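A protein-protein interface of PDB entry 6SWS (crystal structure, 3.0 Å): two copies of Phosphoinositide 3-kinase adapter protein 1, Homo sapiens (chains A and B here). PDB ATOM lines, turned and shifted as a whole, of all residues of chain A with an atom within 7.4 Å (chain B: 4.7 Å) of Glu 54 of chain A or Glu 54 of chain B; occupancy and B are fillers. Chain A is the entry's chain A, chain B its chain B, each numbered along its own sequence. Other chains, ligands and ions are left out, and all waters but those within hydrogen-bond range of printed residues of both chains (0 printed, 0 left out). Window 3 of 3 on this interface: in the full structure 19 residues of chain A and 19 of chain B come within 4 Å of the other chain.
The backbone NH (N) of Val 23 of chain A sits at hydrogen-bond distance from the backbone carbonyl oxygen (O) of Tyr 55 of chain A. The side-chain carboxylate (OE1) of Glu 54 of chain A lies within salt-bridge range of the side-chain amino group (NZ) of Lys 26 of chain A (3.6 Å). OD1 of Asn 53 of chain A sits close to N of Tyr 55 of chain A (3.0 Å). The side-chain hydroxyl of Thr 56 of chain A lies within hydrogen-bond range of the side-chain amide oxygen of Asn 53 of chain A (2.7 Å). The side-chain amide oxygen of Asn 53 of chain B is in hydrogen-bond range of the backbone NH of Tyr 55 of chain B (2.7 Å). The side-chain amide oxygen of Asn 53 of chain B lies within hydrogen-bond range of the backbone NH of Thr 56 of chain B, 2.7 Å away.
Among the printed residues, pairs that only touch across the chains: Asn 53 of chain A with Tyr 55 of chain B (3.7 Å), Glu 54 of chain A with Glu 54 of chain B (3.9 Å) and Tyr 55 of chain A with Asn 53 of chain B (3.5 Å).
Glu 54 of chain B touches one residue of chain A. Printed residues of chain B within 4 Å of Tyr 55 of chain A: Asn 53 (3.5 Å). Of the printed residues of chain A, Tyr 55 of chain B touches Asn 53. Of the printed residues of chain A, Asn 53 of chain B touches Tyr 55 (3.5 Å). Of the printed residues of chain B, Asn 53 of chain A touches Tyr 55. Thr 56 of chain A touches none of the printed residues of chain B. The nearest residue of chain B that does not touch Glu 54 of chain A is Tyr 55 of chain B (4.3 Å).
Along chain B the printed residues that touch a printed residue of chain A span positions 53 to 55. Of the 14 printed residues of chain A, 3 touch a printed residue of chain B. Along chain A the printed residues that touch a printed residue of chain B span positions 53 to 55. Among the printed residues, 3 pairs touch across the chains.
Asn 53 of chain A touches Tyr 55 of chain B, and with the chains exchanged Tyr 55 of chain A touches Asn 53 of chain B. Glu 54 of chain B touches its own counterpart, Glu 54 of chain A. Positions printed for both chains: 25, 26, 27, 53, 54, 55 and 56. Of the 3 pairs that touch across the chains among the printed residues, 3 have their exchanged pair printed and touching as well.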
ATOM      1  N   VAL A  23      -0.377  -5.475  29.697  1.00  0.00           N
ATOM      2  CA  VAL A  23      -1.736  -5.901  29.384  1.00  0.00           C
ATOM      3  C   VAL A  23      -2.144  -7.038  30.316  1.00  0.00           C
ATOM      4  O   VAL A  23      -1.312  -7.842  30.749  1.00  0.00           O
ATOM      5  CB  VAL A  23      -1.830  -6.312  27.899  1.00  0.00           C
ATOM      6  CG1 VAL A  23      -3.227  -6.772  27.540  1.00  0.00           C
ATOM      7  CG2 VAL A  23      -1.422  -5.150  27.015  1.00  0.00           C
ATOM      8  N   ARG A  24      -3.444  -7.099  30.629  1.00  0.00           N
ATOM      9  CA  ARG A  24      -3.994  -8.146  31.486  1.00  0.00           C
ATOM     10  C   ARG A  24      -4.285  -9.446  30.750  1.00  0.00           C
ATOM     11  O   ARG A  24      -4.511 -10.466  31.410  1.00  0.00           O
ATOM     12  CB  ARG A  24      -5.277  -7.665  32.170  1.00  0.00           C
ATOM     13  CG  ARG A  24      -5.050  -6.550  33.157  1.00  0.00           C
ATOM     14  CD  ARG A  24      -6.261  -6.289  34.032  1.00  0.00           C
ATOM     15  NE  ARG A  24      -5.875  -5.580  35.248  1.00  0.00           N
ATOM     16  CZ  ARG A  24      -5.967  -4.265  35.415  1.00  0.00           C
ATOM     17  NH1 ARG A  24      -6.431  -3.496  34.440  1.00  0.00           N
ATOM     18  NH2 ARG A  24      -5.588  -3.716  36.563  1.00  0.00           N
ATOM     19  N   CYS A  25      -4.295  -9.440  29.422  1.00  0.00           N
ATOM     20  CA  CYS A  25      -4.625 -10.616  28.634  1.00  0.00           C
ATOM     21  C   CYS A  25      -3.453 -10.963  27.731  1.00  0.00           C
ATOM     22  O   CYS A  25      -2.734 -10.078  27.258  1.00  0.00           O
ATOM     23  CB  CYS A  25      -5.883 -10.390  27.787  1.00  0.00           C
ATOM     24  SG  CYS A  25      -7.427 -10.446  28.719  1.00  0.00           S
ATOM     25  N   LYS A  26      -3.264 -12.261  27.504  1.00  0.00           N
ATOM     26  CA  LYS A  26      -2.144 -12.717  26.694  1.00  0.00           C
ATOM     27  C   LYS A  26      -2.205 -12.109  25.300  1.00  0.00           C
ATOM     28  O   LYS A  26      -3.274 -11.996  24.694  1.00  0.00           O
ATOM     29  CB  LYS A  26      -2.141 -14.240  26.598  1.00  0.00           C
ATOM     30  CG  LYS A  26      -1.480 -14.938  27.776  1.00  0.00           C
ATOM     31  CD  LYS A  26      -0.950 -16.302  27.370  1.00  0.00           C
ATOM     32  CE  LYS A  26      -0.580 -17.142  28.580  1.00  0.00           C
ATOM     33  NZ  LYS A  26       0.374 -18.223  28.209  1.00  0.00           N
ATOM     34  N   LEU A  27      -1.044 -11.714  24.797  1.00  0.00           N
ATOM     35  CA  LEU A  27      -0.937 -11.122  23.475  1.00  0.00           C
ATOM     36  C   LEU A  27      -0.556 -12.193  22.464  1.00  0.00           C
ATOM     37  O   LEU A  27       0.247 -13.084  22.760  1.00  0.00           O
ATOM     38  CB  LEU A  27       0.096 -10.004  23.464  1.00  0.00           C
ATOM     39  CG  LEU A  27      -0.503  -8.618  23.667  1.00  0.00           C
ATOM     40  CD1 LEU A  27      -1.038  -8.453  25.085  1.00  0.00           C
ATOM     41  CD2 LEU A  27       0.543  -7.609  23.339  1.00  0.00           C
ATOM     42  N   ASP A  28      -1.137 -12.105  21.271  1.00  0.00           N
ATOM     43  CA  ASP A  28      -0.777 -13.015  20.192  1.00  0.00           C
ATOM     44  C   ASP A  28       0.548 -12.553  19.600  1.00  0.00           C
ATOM     45  O   ASP A  28       0.634 -11.465  19.022  1.00  0.00           O
ATOM     46  CB  ASP A  28      -1.877 -13.065  19.135  1.00  0.00           C
ATOM     47  CG  ASP A  28      -1.779 -14.296  18.249  1.00  0.00           C
ATOM     48  OD1 ASP A  28      -0.649 -14.688  17.890  1.00  0.00           O
ATOM     49  OD2 ASP A  28      -2.835 -14.868  17.904  1.00  0.00           O
ATOM     50  N   ASP A  29       1.585 -13.377  19.760  1.00  0.00           N
ATOM     51  CA  ASP A  29       2.905 -13.019  19.256  1.00  0.00           C
ATOM     52  C   ASP A  29       2.914 -12.917  17.737  1.00  0.00           C
ATOM     53  O   ASP A  29       3.633 -12.084  17.176  1.00  0.00           O
ATOM     54  CB  ASP A  29       3.937 -14.046  19.724  1.00  0.00           C
ATOM     55  CG  ASP A  29       5.282 -13.421  20.048  1.00  0.00           C
ATOM     56  OD1 ASP A  29       5.411 -12.186  19.928  1.00  0.00           O
ATOM     57  OD2 ASP A  29       6.210 -14.169  20.423  1.00  0.00           O
ATOM     58  N   VAL A  51       5.699  -6.047  20.323  1.00  0.00           N
ATOM     59  CA  VAL A  51       5.221  -6.924  21.388  1.00  0.00           C
ATOM     60  C   VAL A  51       6.438  -7.514  22.103  1.00  0.00           C
ATOM     61  O   VAL A  51       7.113  -8.422  21.614  1.00  0.00           O
ATOM     62  CB  VAL A  51       4.258  -7.992  20.862  1.00  0.00           C
ATOM     63  CG1 VAL A  51       4.949  -8.942  19.918  1.00  0.00           C
ATOM     64  CG2 VAL A  51       3.714  -8.788  22.026  1.00  0.00           C
ATOM     65  N   GLU A  52       6.748  -6.948  23.265  1.00  0.00           N
ATOM     66  CA  GLU A  52       7.925  -7.382  24.005  1.00  0.00           C
ATOM     67  C   GLU A  52       7.697  -8.728  24.680  1.00  0.00           C
ATOM     68  O   GLU A  52       8.614  -9.557  24.737  1.00  0.00           O
ATOM     69  CB  GLU A  52       8.308  -6.316  25.025  1.00  0.00           C
ATOM     70  CG  GLU A  52       8.611  -4.968  24.396  1.00  0.00           C
ATOM     71  CD  GLU A  52       9.991  -4.909  23.766  1.00  0.00           C
ATOM     72  OE1 GLU A  52      10.663  -5.958  23.701  1.00  0.00           O
ATOM     73  OE2 GLU A  52      10.405  -3.817  23.324  1.00  0.00           O
ATOM     74  N   ASN A  53       6.497  -8.967  25.208  1.00  0.00           N
ATOM     75  CA  ASN A  53       6.169 -10.310  25.684  1.00  0.00           C
ATOM     76  C   ASN A  53       4.656 -10.438  25.807  1.00  0.00           C
ATOM     77  O   ASN A  53       3.906  -9.504  25.508  1.00  0.00           O
ATOM     78  CB  ASN A  53       6.879 -10.643  27.005  1.00  0.00           C
ATOM     79  CG  ASN A  53       6.558  -9.670  28.112  1.00  0.00           C
ATOM     80  OD1 ASN A  53       5.395  -9.402  28.402  1.00  0.00           O
ATOM     81  ND2 ASN A  53       7.594  -9.130  28.737  1.00  0.00           N
ATOM     82  N   GLU A  54       4.217 -11.617  26.269  1.00  0.00           N
ATOM     83  CA  GLU A  54       2.799 -11.960  26.315  1.00  0.00           C
ATOM     84  C   GLU A  54       1.949 -10.890  26.983  1.00  0.00           C
ATOM     85  O   GLU A  54       0.740 -10.826  26.731  1.00  0.00           O
ATOM     86  CB  GLU A  54       2.600 -13.278  27.069  1.00  0.00           C
ATOM     87  CG  GLU A  54       3.175 -14.503  26.391  1.00  0.00           C
ATOM     88  CD  GLU A  54       3.159 -15.719  27.299  1.00  0.00           C
ATOM     89  OE1 GLU A  54       2.778 -15.575  28.480  1.00  0.00           O
ATOM     90  OE2 GLU A  54       3.529 -16.818  26.834  1.00  0.00           O
ATOM     91  N   TYR A  55       2.546 -10.054  27.831  1.00  0.00           N
ATOM     92  CA  TYR A  55       1.812  -9.021  28.542  1.00  0.00           C
ATOM     93  C   TYR A  55       2.370  -7.619  28.331  1.00  0.00           C
ATOM     94  O   TYR A  55       1.812  -6.665  28.885  1.00  0.00           O
ATOM     95  CB  TYR A  55       1.789  -9.338  30.044  1.00  0.00           C
ATOM     96  CG  TYR A  55       1.225 -10.704  30.371  1.00  0.00           C
ATOM     97  CD1 TYR A  55       2.057 -11.813  30.452  1.00  0.00           C
ATOM     98  CD2 TYR A  55      -0.132 -10.884  30.601  1.00  0.00           C
ATOM     99  CE1 TYR A  55       1.555 -13.066  30.749  1.00  0.00           C
ATOM    100  CE2 TYR A  55      -0.645 -12.135  30.902  1.00  0.00           C
ATOM    101  CZ  TYR A  55       0.205 -13.222  30.974  1.00  0.00           C
ATOM    102  OH  TYR A  55      -0.294 -14.469  31.271  1.00  0.00           O
ATOM    103  N   THR A  56       3.442  -7.458  27.554  1.00  0.00           N
ATOM    104  CA  THR A  56       4.145  -6.183  27.465  1.00  0.00           C
ATOM    105  C   THR A  56       4.281  -5.737  26.017  1.00  0.00           C
ATOM    106  O   THR A  56       4.803  -6.489  25.182  1.00  0.00           O
ATOM    107  CB  THR A  56       5.538  -6.273  28.098  1.00  0.00           C
ATOM    108  OG1 THR A  56       5.441  -6.848  29.407  1.00  0.00           O
ATOM    109  CG2 THR A  56       6.168  -4.890  28.195  1.00  0.00           C
ATOM    110  N   ILE A  57       3.835  -4.504  25.746  1.00  0.00           N
ATOM    111  CA  ILE A  57       3.973  -3.834  24.456  1.00  0.00           C
ATOM    112  C   ILE A  57       4.874  -2.622  24.639  1.00  0.00           C
ATOM    113  O   ILE A  57       4.799  -1.936  25.663  1.00  0.00           O
ATOM    114  CB  ILE A  57       2.613  -3.372  23.895  1.00  0.00           C
ATOM    115  CG1 ILE A  57       1.591  -4.494  23.967  1.00  0.00           C
ATOM    116  CG2 ILE A  57       2.758  -2.893  22.454  1.00  0.00           C
ATOM    117  CD1 ILE A  57       0.165  -4.006  23.978  1.00  0.00           C
ATOM    118  N   CYS B  25      13.338 -13.720  31.361  1.00  0.00           N
ATOM    119  CA  CYS B  25      13.093 -15.086  31.802  1.00  0.00           C
ATOM    120  C   CYS B  25      11.832 -15.132  32.655  1.00  0.00           C
ATOM    121  O   CYS B  25      11.666 -14.316  33.567  1.00  0.00           O
ATOM    122  CB  CYS B  25      14.287 -15.621  32.593  1.00  0.00           C
ATOM    123  SG  CYS B  25      15.796 -15.787  31.617  1.00  0.00           S
ATOM    124  N   LYS B  26      10.942 -16.074  32.343  1.00  0.00           N
ATOM    125  CA  LYS B  26       9.733 -16.261  33.134  1.00  0.00           C
ATOM    126  C   LYS B  26      10.097 -16.490  34.594  1.00  0.00           C
ATOM    127  O   LYS B  26      10.903 -17.367  34.917  1.00  0.00           O
ATOM    128  CB  LYS B  26       8.929 -17.443  32.591  1.00  0.00           C
ATOM    129  CG  LYS B  26       7.486 -17.503  33.051  1.00  0.00           C
ATOM    130  CD  LYS B  26       6.721 -18.555  32.267  1.00  0.00           C
ATOM    131  CE  LYS B  26       6.825 -18.308  30.767  1.00  0.00           C
ATOM    132  NZ  LYS B  26       6.135 -19.365  29.973  1.00  0.00           N
ATOM    133  N   LEU B  27       9.510 -15.687  35.474  1.00  0.00           N
ATOM    134  CA  LEU B  27       9.831 -15.768  36.890  1.00  0.00           C
ATOM    135  C   LEU B  27       9.145 -16.956  37.544  1.00  0.00           C
ATOM    136  O   LEU B  27       8.008 -17.299  37.208  1.00  0.00           O
ATOM    137  CB  LEU B  27       9.384 -14.492  37.600  1.00  0.00           C
ATOM    138  CG  LEU B  27      10.316 -13.297  37.762  1.00  0.00           C
ATOM    139  CD1 LEU B  27      11.167 -13.080  36.532  1.00  0.00           C
ATOM    140  CD2 LEU B  27       9.431 -12.105  37.995  1.00  0.00           C
ATOM    141  N   ASN B  53       3.433  -9.978  37.017  1.00  0.00           N
ATOM    142  CA  ASN B  53       3.182 -11.128  36.152  1.00  0.00           C
ATOM    143  C   ASN B  53       4.487 -11.882  35.930  1.00  0.00           C
ATOM    144  O   ASN B  53       5.543 -11.507  36.450  1.00  0.00           O
ATOM    145  CB  ASN B  53       2.526 -10.701  34.829  1.00  0.00           C
ATOM    146  CG  ASN B  53       3.417  -9.814  33.973  1.00  0.00           C
ATOM    147  OD1 ASN B  53       4.619 -10.043  33.846  1.00  0.00           O
ATOM    148  ND2 ASN B  53       2.823  -8.783  33.385  1.00  0.00           N
ATOM    149  N   GLU B  54       4.404 -12.947  35.122  1.00  0.00           N
ATOM    150  CA  GLU B  54       5.537 -13.839  34.890  1.00  0.00           C
ATOM    151  C   GLU B  54       6.779 -13.113  34.396  1.00  0.00           C
ATOM    152  O   GLU B  54       7.873 -13.684  34.435  1.00  0.00           O
ATOM    153  CB  GLU B  54       5.161 -14.924  33.880  1.00  0.00           C
ATOM    154  CG  GLU B  54       3.828 -15.591  34.132  1.00  0.00           C
ATOM    155  CD  GLU B  54       3.403 -16.466  32.973  1.00  0.00           C
ATOM    156  OE1 GLU B  54       4.144 -16.525  31.968  1.00  0.00           O
ATOM    157  OE2 GLU B  54       2.329 -17.090  33.067  1.00  0.00           O
ATOM    158  N   TYR B  55       6.640 -11.873  33.928  1.00  0.00           N
ATOM    159  CA  TYR B  55       7.777 -11.102  33.459  1.00  0.00           C
ATOM    160  C   TYR B  55       7.897  -9.744  34.133  1.00  0.00           C
ATOM    161  O   TYR B  55       8.844  -9.011  33.834  1.00  0.00           O
ATOM    162  CB  TYR B  55       7.703 -10.885  31.938  1.00  0.00           C
ATOM    163  CG  TYR B  55       7.644 -12.148  31.104  1.00  0.00           C
ATOM    164  CD1 TYR B  55       6.438 -12.803  30.882  1.00  0.00           C
ATOM    165  CD2 TYR B  55       8.790 -12.672  30.520  1.00  0.00           C
ATOM    166  CE1 TYR B  55       6.379 -13.950  30.113  1.00  0.00           C
ATOM    167  CE2 TYR B  55       8.741 -13.817  29.750  1.00  0.00           C
ATOM    168  CZ  TYR B  55       7.533 -14.453  29.549  1.00  0.00           C
ATOM    169  OH  TYR B  55       7.486 -15.593  28.782  1.00  0.00           O
ATOM    170  N   THR B  56       6.982  -9.389  35.033  1.00  0.00           N
ATOM    171  CA  THR B  56       6.899  -8.030  35.548  1.00  0.00           C
ATOM    172  C   THR B  56       6.892  -8.040  37.067  1.00  0.00           C
ATOM    173  O   THR B  56       6.057  -8.714  37.683  1.00  0.00           O
ATOM    174  CB  THR B  56       5.644  -7.317  35.032  1.00  0.00           C
ATOM    175  OG1 THR B  56       5.667  -7.271  33.600  1.00  0.00           O
ATOM    176  CG2 THR B  56       5.567  -5.901  35.586  1.00  0.00           C
